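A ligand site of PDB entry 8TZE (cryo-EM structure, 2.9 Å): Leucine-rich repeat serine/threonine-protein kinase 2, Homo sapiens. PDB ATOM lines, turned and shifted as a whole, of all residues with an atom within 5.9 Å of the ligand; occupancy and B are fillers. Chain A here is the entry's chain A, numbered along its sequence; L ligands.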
ATOM      1  N   LEU A1885      13.617 -11.240 -13.800  1.00  0.00           N
ATOM      2  CA  LEU A1885      13.220  -9.863 -13.525  1.00  0.00           C
ATOM      3  C   LEU A1885      11.807  -9.840 -12.960  1.00  0.00           C
ATOM      4  O   LEU A1885      10.875 -10.364 -13.562  1.00  0.00           O
ATOM      5  CB  LEU A1885      13.299  -9.030 -14.803  1.00  0.00           C
ATOM      6  CG  LEU A1885      14.456  -8.034 -14.870  1.00  0.00           C
ATOM      7  CD1 LEU A1885      14.246  -7.054 -15.996  1.00  0.00           C
ATOM      8  CD2 LEU A1885      14.589  -7.303 -13.544  1.00  0.00           C
ATOM      9  N   GLY A1886      11.660  -9.209 -11.789  1.00  0.00           N
ATOM     10  CA  GLY A1886      10.375  -9.159 -11.130  1.00  0.00           C
ATOM     11  C   GLY A1886       9.917 -10.444 -10.494  1.00  0.00           C
ATOM     12  O   GLY A1886       8.713 -10.663 -10.378  1.00  0.00           O
ATOM     13  N   PHE A1890       6.472 -10.066 -15.577  1.00  0.00           N
ATOM     14  CA  PHE A1890       7.011  -9.794 -16.908  1.00  0.00           C
ATOM     15  C   PHE A1890       7.246 -11.070 -17.701  1.00  0.00           C
ATOM     16  O   PHE A1890       7.663 -11.015 -18.864  1.00  0.00           O
ATOM     17  CB  PHE A1890       8.305  -8.976 -16.827  1.00  0.00           C
ATOM     18  CG  PHE A1890       8.264  -7.858 -15.830  1.00  0.00           C
ATOM     19  CD1 PHE A1890       7.532  -6.708 -16.095  1.00  0.00           C
ATOM     20  CD2 PHE A1890       8.964  -7.935 -14.644  1.00  0.00           C
ATOM     21  CE1 PHE A1890       7.488  -5.674 -15.184  1.00  0.00           C
ATOM     22  CE2 PHE A1890       8.919  -6.909 -13.728  1.00  0.00           C
ATOM     23  CZ  PHE A1890       8.190  -5.773 -13.995  1.00  0.00           C
ATOM     24  N   VAL A1893      11.576 -12.770 -18.468  1.00  0.00           N
ATOM     25  CA  VAL A1893      12.448 -11.618 -18.633  1.00  0.00           C
ATOM     26  C   VAL A1893      13.588 -11.763 -17.629  1.00  0.00           C
ATOM     27  O   VAL A1893      13.357 -11.990 -16.432  1.00  0.00           O
ATOM     28  CB  VAL A1893      11.695 -10.297 -18.443  1.00  0.00           C
ATOM     29  CG1 VAL A1893      12.649  -9.123 -18.518  1.00  0.00           C
ATOM     30  CG2 VAL A1893      10.623 -10.149 -19.498  1.00  0.00           C
ATOM     31  N   ARG A1895      17.733 -10.461 -16.372  1.00  0.00           N
ATOM     32  CA  ARG A1895      18.801  -9.478 -16.410  1.00  0.00           C
ATOM     33  C   ARG A1895      20.005 -10.059 -17.147  1.00  0.00           C
ATOM     34  O   ARG A1895      20.347 -11.230 -16.960  1.00  0.00           O
ATOM     35  CB  ARG A1895      19.203  -9.067 -14.994  1.00  0.00           C
ATOM     36  CG  ARG A1895      18.134  -8.323 -14.229  1.00  0.00           C
ATOM     37  CD  ARG A1895      18.585  -8.034 -12.802  1.00  0.00           C
ATOM     38  NE  ARG A1895      17.566  -7.330 -12.028  1.00  0.00           N
ATOM     39  CZ  ARG A1895      17.481  -6.011 -11.924  1.00  0.00           C
ATOM     40  NH1 ARG A1895      18.349  -5.210 -12.519  1.00  0.00           N
ATOM     41  NH2 ARG A1895      16.495  -5.480 -11.216  1.00  0.00           N
ATOM     42  N   ALA A1904      17.499  -6.117 -20.489  1.00  0.00           N
ATOM     43  CA  ALA A1904      16.451  -7.092 -20.224  1.00  0.00           C
ATOM     44  C   ALA A1904      16.355  -8.041 -21.406  1.00  0.00           C
ATOM     45  O   ALA A1904      16.459  -7.625 -22.563  1.00  0.00           O
ATOM     46  CB  ALA A1904      15.102  -6.409 -19.977  1.00  0.00           C
ATOM     47  N   VAL A1905      16.159  -9.334 -21.117  1.00  0.00           N
ATOM     48  CA  VAL A1905      16.202 -10.393 -22.113  1.00  0.00           C
ATOM     49  C   VAL A1905      14.904 -11.184 -22.027  1.00  0.00           C
ATOM     50  O   VAL A1905      14.574 -11.740 -20.969  1.00  0.00           O
ATOM     51  CB  VAL A1905      17.414 -11.302 -21.906  1.00  0.00           C
ATOM     52  CG1 VAL A1905      17.317 -12.508 -22.799  1.00  0.00           C
ATOM     53  CG2 VAL A1905      18.694 -10.544 -22.199  1.00  0.00           C
ATOM     54  N   LYS A1906      14.161 -11.240 -23.133  1.00  0.00           N
ATOM     55  CA  LYS A1906      12.947 -12.038 -23.212  1.00  0.00           C
ATOM     56  C   LYS A1906      13.207 -13.289 -24.033  1.00  0.00           C
ATOM     57  O   LYS A1906      13.763 -13.207 -25.139  1.00  0.00           O
ATOM     58  CB  LYS A1906      11.817 -11.223 -23.840  1.00  0.00           C
ATOM     59  CG  LYS A1906      10.502 -11.977 -23.941  1.00  0.00           C
ATOM     60  CD  LYS A1906       9.452 -11.139 -24.642  1.00  0.00           C
ATOM     61  CE  LYS A1906       8.112 -11.832 -24.645  1.00  0.00           C
ATOM     62  NZ  LYS A1906       7.031 -10.922 -25.131  1.00  0.00           N
ATOM     63  N   GLU A1920       6.448  -9.971 -32.950  1.00  0.00           N
ATOM     64  CA  GLU A1920       6.896  -8.903 -32.066  1.00  0.00           C
ATOM     65  C   GLU A1920       7.999  -8.087 -32.712  1.00  0.00           C
ATOM     66  O   GLU A1920       8.076  -6.869 -32.499  1.00  0.00           O
ATOM     67  CB  GLU A1920       7.369  -9.494 -30.735  1.00  0.00           C
ATOM     68  CG  GLU A1920       7.573  -8.459 -29.651  1.00  0.00           C
ATOM     69  CD  GLU A1920       7.483  -9.052 -28.266  1.00  0.00           C
ATOM     70  OE1 GLU A1920       7.319 -10.289 -28.154  1.00  0.00           O
ATOM     71  OE2 GLU A1920       7.580  -8.287 -27.283  1.00  0.00           O
ATOM     72  N   VAL A1923       6.365  -5.686 -35.090  1.00  0.00           N
ATOM     73  CA  VAL A1923       5.802  -4.567 -34.345  1.00  0.00           C
ATOM     74  C   VAL A1923       6.895  -3.612 -33.892  1.00  0.00           C
ATOM     75  O   VAL A1923       6.773  -2.386 -34.025  1.00  0.00           O
ATOM     76  CB  VAL A1923       4.961  -5.079 -33.155  1.00  0.00           C
ATOM     77  CG1 VAL A1923       4.510  -3.919 -32.297  1.00  0.00           C
ATOM     78  CG2 VAL A1923       3.774  -5.875 -33.651  1.00  0.00           C
ATOM     79  N   LEU A1924       7.996  -4.150 -33.344  1.00  0.00           N
ATOM     80  CA  LEU A1924       8.976  -3.325 -32.648  1.00  0.00           C
ATOM     81  C   LEU A1924       9.870  -2.552 -33.610  1.00  0.00           C
ATOM     82  O   LEU A1924      10.223  -1.397 -33.345  1.00  0.00           O
ATOM     83  CB  LEU A1924       9.829  -4.194 -31.726  1.00  0.00           C
ATOM     84  CG  LEU A1924       9.210  -4.598 -30.388  1.00  0.00           C
ATOM     85  CD1 LEU A1924      10.045  -5.690 -29.738  1.00  0.00           C
ATOM     86  CD2 LEU A1924       9.093  -3.397 -29.480  1.00  0.00           C
ATOM     87  N   LEU A1927       8.814   0.995 -34.656  1.00  0.00           N
ATOM     88  CA  LEU A1927       8.402   1.913 -33.591  1.00  0.00           C
ATOM     89  C   LEU A1927       9.644   2.546 -32.993  1.00  0.00           C
ATOM     90  O   LEU A1927      10.378   1.908 -32.242  1.00  0.00           O
ATOM     91  CB  LEU A1927       7.587   1.177 -32.537  1.00  0.00           C
ATOM     92  CG  LEU A1927       6.217   0.659 -32.984  1.00  0.00           C
ATOM     93  CD1 LEU A1927       5.563  -0.134 -31.867  1.00  0.00           C
ATOM     94  CD2 LEU A1927       5.338   1.825 -33.416  1.00  0.00           C
ATOM     95  N   LEU A1932       8.539   4.764 -25.740  1.00  0.00           N
ATOM     96  CA  LEU A1932       8.368   3.324 -25.863  1.00  0.00           C
ATOM     97  C   LEU A1932       9.708   2.638 -25.650  1.00  0.00           C
ATOM     98  O   LEU A1932      10.749   3.160 -26.054  1.00  0.00           O
ATOM     99  CB  LEU A1932       7.796   2.944 -27.228  1.00  0.00           C
ATOM    100  CG  LEU A1932       6.584   3.725 -27.720  1.00  0.00           C
ATOM    101  CD1 LEU A1932       6.217   3.278 -29.126  1.00  0.00           C
ATOM    102  CD2 LEU A1932       5.404   3.561 -26.781  1.00  0.00           C
ATOM    103  N   ILE A1933       9.684   1.474 -24.990  1.00  0.00           N
ATOM    104  CA  ILE A1933      10.918   0.752 -24.714  1.00  0.00           C
ATOM    105  C   ILE A1933      11.586   0.385 -26.032  1.00  0.00           C
ATOM    106  O   ILE A1933      10.936  -0.068 -26.979  1.00  0.00           O
ATOM    107  CB  ILE A1933      10.634  -0.479 -23.839  1.00  0.00           C
ATOM    108  CG1 ILE A1933      11.930  -1.225 -23.542  1.00  0.00           C
ATOM    109  CG2 ILE A1933       9.623  -1.397 -24.504  1.00  0.00           C
ATOM    110  CD1 ILE A1933      11.860  -2.086 -22.310  1.00  0.00           C
ATOM    111  N   LEU A1945      14.815 -11.612 -27.368  1.00  0.00           N
ATOM    112  CA  LEU A1945      14.744 -10.171 -27.576  1.00  0.00           C
ATOM    113  C   LEU A1945      15.538  -9.488 -26.482  1.00  0.00           C
ATOM    114  O   LEU A1945      15.300  -9.738 -25.288  1.00  0.00           O
ATOM    115  CB  LEU A1945      13.297  -9.670 -27.561  1.00  0.00           C
ATOM    116  CG  LEU A1945      12.402  -9.950 -28.765  1.00  0.00           C
ATOM    117  CD1 LEU A1945      10.984  -9.483 -28.470  1.00  0.00           C
ATOM    118  CD2 LEU A1945      12.940  -9.285 -30.006  1.00  0.00           C
ATOM    119  N   MET A1947      16.319  -5.897 -24.895  1.00  0.00           N
ATOM    120  CA  MET A1947      15.827  -4.524 -24.806  1.00  0.00           C
ATOM    121  C   MET A1947      16.520  -3.802 -23.658  1.00  0.00           C
ATOM    122  O   MET A1947      17.182  -4.420 -22.818  1.00  0.00           O
ATOM    123  CB  MET A1947      14.313  -4.480 -24.609  1.00  0.00           C
ATOM    124  CG  MET A1947      13.554  -5.628 -25.234  1.00  0.00           C
ATOM    125  SD  MET A1947      12.836  -5.208 -26.831  1.00  0.00           S
ATOM    126  CE  MET A1947      11.667  -3.931 -26.358  1.00  0.00           C
ATOM    127  N   GLU A1948      16.353  -2.485 -23.630  1.00  0.00           N
ATOM    128  CA  GLU A1948      16.963  -1.673 -22.581  1.00  0.00           C
ATOM    129  C   GLU A1948      16.321  -1.983 -21.229  1.00  0.00           C
ATOM    130  O   GLU A1948      15.152  -2.360 -21.130  1.00  0.00           O
ATOM    131  CB  GLU A1948      16.822  -0.194 -22.914  1.00  0.00           C
ATOM    132  CG  GLU A1948      15.385   0.282 -23.018  1.00  0.00           C
ATOM    133  CD  GLU A1948      15.296   1.750 -23.391  1.00  0.00           C
ATOM    134  OE1 GLU A1948      16.174   2.520 -22.952  1.00  0.00           O
ATOM    135  OE2 GLU A1948      14.348   2.129 -24.100  1.00  0.00           O
ATOM    136  N   LEU A1949      17.106  -1.807 -20.163  1.00  0.00           N
ATOM    137  CA  LEU A1949      16.687  -2.132 -18.819  1.00  0.00           C
ATOM    138  C   LEU A1949      16.241  -0.879 -18.083  1.00  0.00           C
ATOM    139  O   LEU A1949      16.944   0.135 -18.101  1.00  0.00           O
ATOM    140  CB  LEU A1949      17.808  -2.823 -18.040  1.00  0.00           C
ATOM    141  CG  LEU A1949      17.513  -3.170 -16.585  1.00  0.00           C
ATOM    142  CD1 LEU A1949      16.503  -4.287 -16.493  1.00  0.00           C
ATOM    143  CD2 LEU A1949      18.792  -3.534 -15.853  1.00  0.00           C
ATOM    144  N   ALA A1950      15.087  -0.942 -17.431  1.00  0.00           N
ATOM    145  CA  ALA A1950      14.591   0.143 -16.597  1.00  0.00           C
ATOM    146  C   ALA A1950      15.223   0.006 -15.215  1.00  0.00           C
ATOM    147  O   ALA A1950      14.991  -0.987 -14.518  1.00  0.00           O
ATOM    148  CB  ALA A1950      13.066   0.113 -16.514  1.00  0.00           C
ATOM    149  N   SER A1951      16.011   1.003 -14.821  1.00  0.00           N
ATOM    150  CA  SER A1951      16.722   0.930 -13.542  1.00  0.00           C
ATOM    151  C   SER A1951      15.770   0.906 -12.358  1.00  0.00           C
ATOM    152  O   SER A1951      15.994   0.152 -11.403  1.00  0.00           O
ATOM    153  CB  SER A1951      17.678   2.112 -13.418  1.00  0.00           C
ATOM    154  OG  SER A1951      18.670   2.076 -14.426  1.00  0.00           O
ATOM    155  N   GLY A1953      12.524   0.021 -12.189  1.00  0.00           N
ATOM    156  CA  GLY A1953      11.411  -0.895 -12.191  1.00  0.00           C
ATOM    157  C   GLY A1953      10.167  -0.307 -12.827  1.00  0.00           C
ATOM    158  O   GLY A1953      10.223   0.648 -13.615  1.00  0.00           O
ATOM    159  N   SER A1954       9.017  -0.877 -12.485  1.00  0.00           N
ATOM    160  CA  SER A1954       7.738  -0.479 -13.038  1.00  0.00           C
ATOM    161  C   SER A1954       7.017   0.498 -12.106  1.00  0.00           C
ATOM    162  O   SER A1954       7.382   0.665 -10.946  1.00  0.00           O
ATOM    163  CB  SER A1954       6.854  -1.699 -13.283  1.00  0.00           C
ATOM    164  OG  SER A1954       6.627  -2.418 -12.085  1.00  0.00           O
ATOM    165  N   LEU A1985       1.784   5.924 -30.426  1.00  0.00           N
ATOM    166  CA  LEU A1985       1.183   4.667 -30.878  1.00  0.00           C
ATOM    167  C   LEU A1985      -0.070   4.918 -31.697  1.00  0.00           C
ATOM    168  O   LEU A1985      -0.312   4.221 -32.695  1.00  0.00           O
ATOM    169  CB  LEU A1985       0.870   3.764 -29.685  1.00  0.00           C
ATOM    170  CG  LEU A1985       2.050   3.087 -29.003  1.00  0.00           C
ATOM    171  CD1 LEU A1985       1.578   2.257 -27.823  1.00  0.00           C
ATOM    172  CD2 LEU A1985       2.794   2.220 -29.998  1.00  0.00           C
ATOM    173  N   ILE A1990      -1.763   2.033 -34.205  1.00  0.00           N
ATOM    174  CA  ILE A1990      -1.389   0.918 -33.336  1.00  0.00           C
ATOM    175  C   ILE A1990      -2.097   1.104 -32.003  1.00  0.00           C
ATOM    176  O   ILE A1990      -2.071   2.204 -31.422  1.00  0.00           O
ATOM    177  CB  ILE A1990       0.137   0.843 -33.152  1.00  0.00           C
ATOM    178  CG1 ILE A1990       0.785   0.270 -34.406  1.00  0.00           C
ATOM    179  CG2 ILE A1990       0.489  -0.003 -31.944  1.00  0.00           C
ATOM    180  CD1 ILE A1990       2.262   0.036 -34.274  1.00  0.00           C
ATOM    181  N   ILE A1991      -2.738   0.044 -31.511  1.00  0.00           N
ATOM    182  CA  ILE A1991      -3.563   0.103 -30.321  1.00  0.00           C
ATOM    183  C   ILE A1991      -2.856  -0.628 -29.189  1.00  0.00           C
ATOM    184  O   ILE A1991      -2.453  -1.785 -29.343  1.00  0.00           O
ATOM    185  CB  ILE A1991      -4.953  -0.506 -30.584  1.00  0.00           C
ATOM    186  CG1 ILE A1991      -5.716   0.346 -31.585  1.00  0.00           C
ATOM    187  CG2 ILE A1991      -5.754  -0.640 -29.291  1.00  0.00           C
ATOM    188  CD1 ILE A1991      -6.970  -0.309 -32.104  1.00  0.00           C
ATOM    189  N   TYR A1992      -2.700   0.049 -28.053  1.00  0.00           N
ATOM    190  CA  TYR A1992      -2.183  -0.552 -26.826  1.00  0.00           C
ATOM    191  C   TYR A1992      -3.391  -1.034 -26.025  1.00  0.00           C
ATOM    192  O   TYR A1992      -4.045  -0.255 -25.334  1.00  0.00           O
ATOM    193  CB  TYR A1992      -1.333   0.433 -26.042  1.00  0.00           C
ATOM    194  CG  TYR A1992      -0.420  -0.238 -25.058  1.00  0.00           C
ATOM    195  CD1 TYR A1992       0.875  -0.587 -25.417  1.00  0.00           C
ATOM    196  CD2 TYR A1992      -0.846  -0.512 -23.771  1.00  0.00           C
ATOM    197  CE1 TYR A1992       1.714  -1.198 -24.519  1.00  0.00           C
ATOM    198  CE2 TYR A1992      -0.009  -1.132 -22.868  1.00  0.00           C
ATOM    199  CZ  TYR A1992       1.271  -1.475 -23.243  1.00  0.00           C
ATOM    200  OH  TYR A1992       2.102  -2.087 -22.351  1.00  0.00           O
ATOM    201  N   ARG A1993      -3.669  -2.337 -26.111  1.00  0.00           N
ATOM    202  CA  ARG A1993      -4.944  -2.857 -25.625  1.00  0.00           C
ATOM    203  C   ARG A1993      -5.120  -2.678 -24.130  1.00  0.00           C
ATOM    204  O   ARG A1993      -6.164  -2.207 -23.669  1.00  0.00           O
ATOM    205  CB  ARG A1993      -5.082  -4.338 -26.012  1.00  0.00           C
ATOM    206  CG  ARG A1993      -5.278  -4.562 -27.497  1.00  0.00           C
ATOM    207  CD  ARG A1993      -5.094  -6.030 -27.866  1.00  0.00           C
ATOM    208  NE  ARG A1993      -6.189  -6.866 -27.376  1.00  0.00           N
ATOM    209  CZ  ARG A1993      -7.312  -7.091 -28.037  1.00  0.00           C
ATOM    210  NH1 ARG A1993      -7.532  -6.553 -29.224  1.00  0.00           N
ATOM    211  NH2 ARG A1993      -8.233  -7.875 -27.494  1.00  0.00           N
ATOM    212  N   LEU A2001       7.253   1.505 -17.319  1.00  0.00           N
ATOM    213  CA  LEU A2001       8.587   1.306 -16.769  1.00  0.00           C
ATOM    214  C   LEU A2001       9.231   2.658 -16.483  1.00  0.00           C
ATOM    215  O   LEU A2001       9.096   3.605 -17.251  1.00  0.00           O
ATOM    216  CB  LEU A2001       9.462   0.506 -17.742  1.00  0.00           C
ATOM    217  CG  LEU A2001       9.105  -0.963 -17.943  1.00  0.00           C
ATOM    218  CD1 LEU A2001       9.949  -1.552 -19.050  1.00  0.00           C
ATOM    219  CD2 LEU A2001       9.291  -1.744 -16.661  1.00  0.00           C
ATOM    220  N   ILE A2015       6.494   3.043 -22.051  1.00  0.00           N
ATOM    221  CA  ILE A2015       5.435   2.055 -22.119  1.00  0.00           C
ATOM    222  C   ILE A2015       6.013   0.747 -22.656  1.00  0.00           C
ATOM    223  O   ILE A2015       6.716   0.735 -23.668  1.00  0.00           O
ATOM    224  CB  ILE A2015       4.277   2.545 -22.996  1.00  0.00           C
ATOM    225  CG1 ILE A2015       3.838   3.948 -22.569  1.00  0.00           C
ATOM    226  CG2 ILE A2015       3.100   1.600 -22.910  1.00  0.00           C
ATOM    227  CD1 ILE A2015       2.827   4.565 -23.499  1.00  0.00           C
ATOM    228  N   ALA A2016       5.699  -0.353 -21.972  1.00  0.00           N
ATOM    229  CA  ALA A2016       6.188  -1.667 -22.368  1.00  0.00           C
ATOM    230  C   ALA A2016       5.041  -2.660 -22.355  1.00  0.00           C
ATOM    231  O   ALA A2016       4.118  -2.532 -21.551  1.00  0.00           O
ATOM    232  CB  ALA A2016       7.321  -2.134 -21.440  1.00  0.00           C
ATOM    233  N   ASP A2017       5.102  -3.641 -23.248  1.00  0.00           N
ATOM    234  CA  ASP A2017       4.115  -4.714 -23.316  1.00  0.00           C
ATOM    235  C   ASP A2017       4.835  -6.044 -23.247  1.00  0.00           C
ATOM    236  O   ASP A2017       5.323  -6.545 -24.270  1.00  0.00           O
ATOM    237  CB  ASP A2017       3.287  -4.613 -24.588  1.00  0.00           C
ATOM    238  CG  ASP A2017       2.091  -5.534 -24.591  1.00  0.00           C
ATOM    239  OD1 ASP A2017       1.867  -6.227 -23.570  1.00  0.00           O
ATOM    240  OD2 ASP A2017       1.370  -5.576 -25.604  1.00  0.00           O
ATOM    241  N   TYR A2018       4.895  -6.630 -22.060  1.00  0.00           N
ATOM    242  CA  TYR A2018       5.660  -7.843 -21.811  1.00  0.00           C
ATOM    243  C   TYR A2018       4.955  -9.046 -22.412  1.00  0.00           C
ATOM    244  O   TYR A2018       3.885  -8.932 -23.034  1.00  0.00           O
ATOM    245  CB  TYR A2018       5.873  -8.023 -20.309  1.00  0.00           C
ATOM    246  CG  TYR A2018       5.989  -6.720 -19.546  1.00  0.00           C
ATOM    247  CD1 TYR A2018       7.116  -5.924 -19.664  1.00  0.00           C
ATOM    248  CD2 TYR A2018       4.953  -6.284 -18.734  1.00  0.00           C
ATOM    249  CE1 TYR A2018       7.215  -4.731 -18.978  1.00  0.00           C
ATOM    250  CE2 TYR A2018       5.042  -5.102 -18.048  1.00  0.00           C
ATOM    251  CZ  TYR A2018       6.175  -4.332 -18.171  1.00  0.00           C
ATOM    252  OH  TYR A2018       6.259  -3.145 -17.478  1.00  0.00           O
HETATM  253  C1  LIG L   1       5.047  -2.301 -27.516  1.00  0.00           C
HETATM  254  C2  LIG L   1       4.302  -4.376 -28.528  1.00  0.00           C
HETATM  255  C3  LIG L   1       2.905  -2.288 -29.055  1.00  0.00           C
HETATM  256  C4  LIG L   1      -0.125  -3.733 -30.275  1.00  0.00           C
HETATM  257  C5  LIG L   1       6.266  -4.393 -27.121  1.00  0.00           C
HETATM  258  C6  LIG L   1       6.103  -3.018 -26.928  1.00  0.00           C
HETATM  259  C7  LIG L   1       4.122  -3.004 -28.346  1.00  0.00           C
HETATM  260  C8  LIG L   1       5.367  -5.063 -27.926  1.00  0.00           C
HETATM  261  C9  LIG L   1       1.267  -3.074 -30.251  1.00  0.00           C
HETATM  262  N1  LIG L   1       7.389  -5.130 -26.483  1.00  0.00           N
HETATM  263  C10 LIG L   1      12.147  -7.831 -22.582  1.00  0.00           C
HETATM  264  C11 LIG L   1      11.005  -7.073 -23.251  1.00  0.00           C
HETATM  265  C12 LIG L   1      10.427  -5.995 -22.604  1.00  0.00           C
HETATM  266  C13 LIG L   1       9.394  -5.300 -23.202  1.00  0.00           C
HETATM  267  C14 LIG L   1       8.927  -5.693 -24.448  1.00  0.00           C
HETATM  268  C15 LIG L   1       9.503  -6.779 -25.090  1.00  0.00           C
HETATM  269  C16 LIG L   1      10.546  -7.464 -24.492  1.00  0.00           C
HETATM  270  C17 LIG L   1       7.769  -4.899 -25.082  1.00  0.00           C
HETATM  271  C18 LIG L   1      -0.224  -3.725 -28.131  1.00  0.00           C
HETATM  272  C19 LIG L   1       1.121  -2.990 -28.052  1.00  0.00           C
HETATM  273  C20 LIG L   1      -1.470  -5.047 -29.260  1.00  0.00           C
HETATM  274  C21 LIG L   1       4.936  -0.791 -27.251  1.00  0.00           C
HETATM  275  C22 LIG L   1      10.931  -5.545 -21.225  1.00  0.00           C
HETATM  276  C23 LIG L   1      11.312  -5.178 -20.157  1.00  0.00           C
HETATM  277  C24 LIG L   1      11.801  -4.703 -18.780  1.00  0.00           C
HETATM  278  C25 LIG L   1      11.220  -5.167 -17.616  1.00  0.00           C
HETATM  279  C26 LIG L   1      11.696  -4.708 -16.455  1.00  0.00           C
HETATM  280  C27 LIG L   1      12.782  -3.778 -16.397  1.00  0.00           C
HETATM  281  C28 LIG L   1      11.434  -4.883 -15.057  1.00  0.00           C
HETATM  282  C29 LIG L   1      12.892  -3.768 -18.691  1.00  0.00           C
HETATM  283  F1  LIG L   1       3.709  -0.469 -26.750  1.00  0.00           F
HETATM  284  F2  LIG L   1       5.894  -0.430 -26.350  1.00  0.00           F
HETATM  285  F3  LIG L   1       5.148  -0.110 -28.418  1.00  0.00           F
HETATM  286  N2  LIG L   1       1.885  -3.146 -29.087  1.00  0.00           N
HETATM  287  N3  LIG L   1      -0.300  -4.487 -29.202  1.00  0.00           N
HETATM  288  N4  LIG L   1      12.892  -3.625 -14.985  1.00  0.00           N
HETATM  289  N5  LIG L   1      12.104  -4.277 -14.161  1.00  0.00           N
HETATM  290  N6  LIG L   1      13.383  -3.297 -17.484  1.00  0.00           N
HETATM  291  O1  LIG L   1       7.180  -4.114 -24.418  1.00  0.00           O
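The backbone carbonyl oxygen (O) of Ile 2015 lies close to a fluorine (F2) of the ligand, 3.0 Å away.
Residues that only touch the ligand: Tyr 1992 (3.1 Å), Ala 2016 (3.3 Å), Leu 1949 (3.4 Å), Leu 1927 (3.5 Å), Phe 1890 (3.5 Å), Leu 1885 (3.5 Å), Met 1947 (3.5 Å), Ile 1990 (3.6 Å), Glu 1948 (3.6 Å), Leu 1932 (3.6 Å), Leu 1985 (3.6 Å), Lys 1906 (3.6 Å), Ile 1933 (3.7 Å), Leu 2001 (3.7 Å), Ala 1904 (3.7 Å), Val 1923 (3.8 Å), Leu 1924 (3.8 Å) and Gly 1953 (3.97 Å).
Hydrophobic or aromatic side chains within 4 Å of the ligand: Leu 1885, Phe 1890, Ala 1904, Val 1923, Leu 1924, Leu 1927, Leu 1932, Ile 1933, Met 1947, Leu 1949, Ala 1950, Leu 1985, Ile 1990, Tyr 1992, Leu 2001 and Ala 2016.
Within 4 Å of the ligand: Leu 1885, Phe 1890, Ala 1904, Lys 1906, Glu 1920, Val 1923, Leu 1924, Leu 1927, Leu 1932, Ile 1933, Met 1947, Glu 1948, Leu 1949, Ala 1950, Gly 1953, Leu 1985, Ile 1990, Ile 1991, Tyr 1992, Leu 2001, Ile 2015, Ala 2016 and Asp 2017.
The backbone NH (N) of Asp 2017 sits at hydrogen-bond distance from an oxygen (O1) of the ligand.
O of Asp 2017 lies close to N1 of the ligand (3.3 Å).
The backbone NH of Ala 1950 is in hydrogen-bond range of a nitrogen (N6) of the ligand (2.9 Å).
A nitrogen (N4) of the ligand is in hydrogen-bond range of the backbone carbonyl oxygen (O) of Ala 1950.
A nitrogen (N3) of the ligand lies close to the backbone carbonyl oxygen (O) of Ile 1991, at 3.5 Å.
OE2 of Glu 1920 sits at hydrogen-bond distance from N1 of the ligand (3.3 Å).
The side-chain hydroxyl (OH) of Tyr 1992 lies close to the backbone NH (N) of Asp 2017, at 3.5 Å.
The backbone carbonyl oxygen (O) of Ile 2015 is in hydrogen-bond range of the backbone NH (N) of Ile 1933.
The side-chain carboxylate (OE1) of Glu 1920 is in salt-bridge range of the side-chain amino group (NZ) of Lys 1906 (3.1 Å).
The backbone NH (N) of Leu 1885 sits at hydrogen-bond distance from the backbone carbonyl oxygen (O) of Val 1893, at 2.7 Å.
The backbone carbonyl oxygen of Met 1947 sits at hydrogen-bond distance from the backbone NH of Ala 1904 (2.9 Å).
The backbone carbonyl oxygen (O) of Leu 1985 is in hydrogen-bond range of the backbone NH (N) of Ile 1990, at 3.0 Å.
N of Lys 1906 lies within hydrogen-bond range of O of Leu 1945 (2.9 Å).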
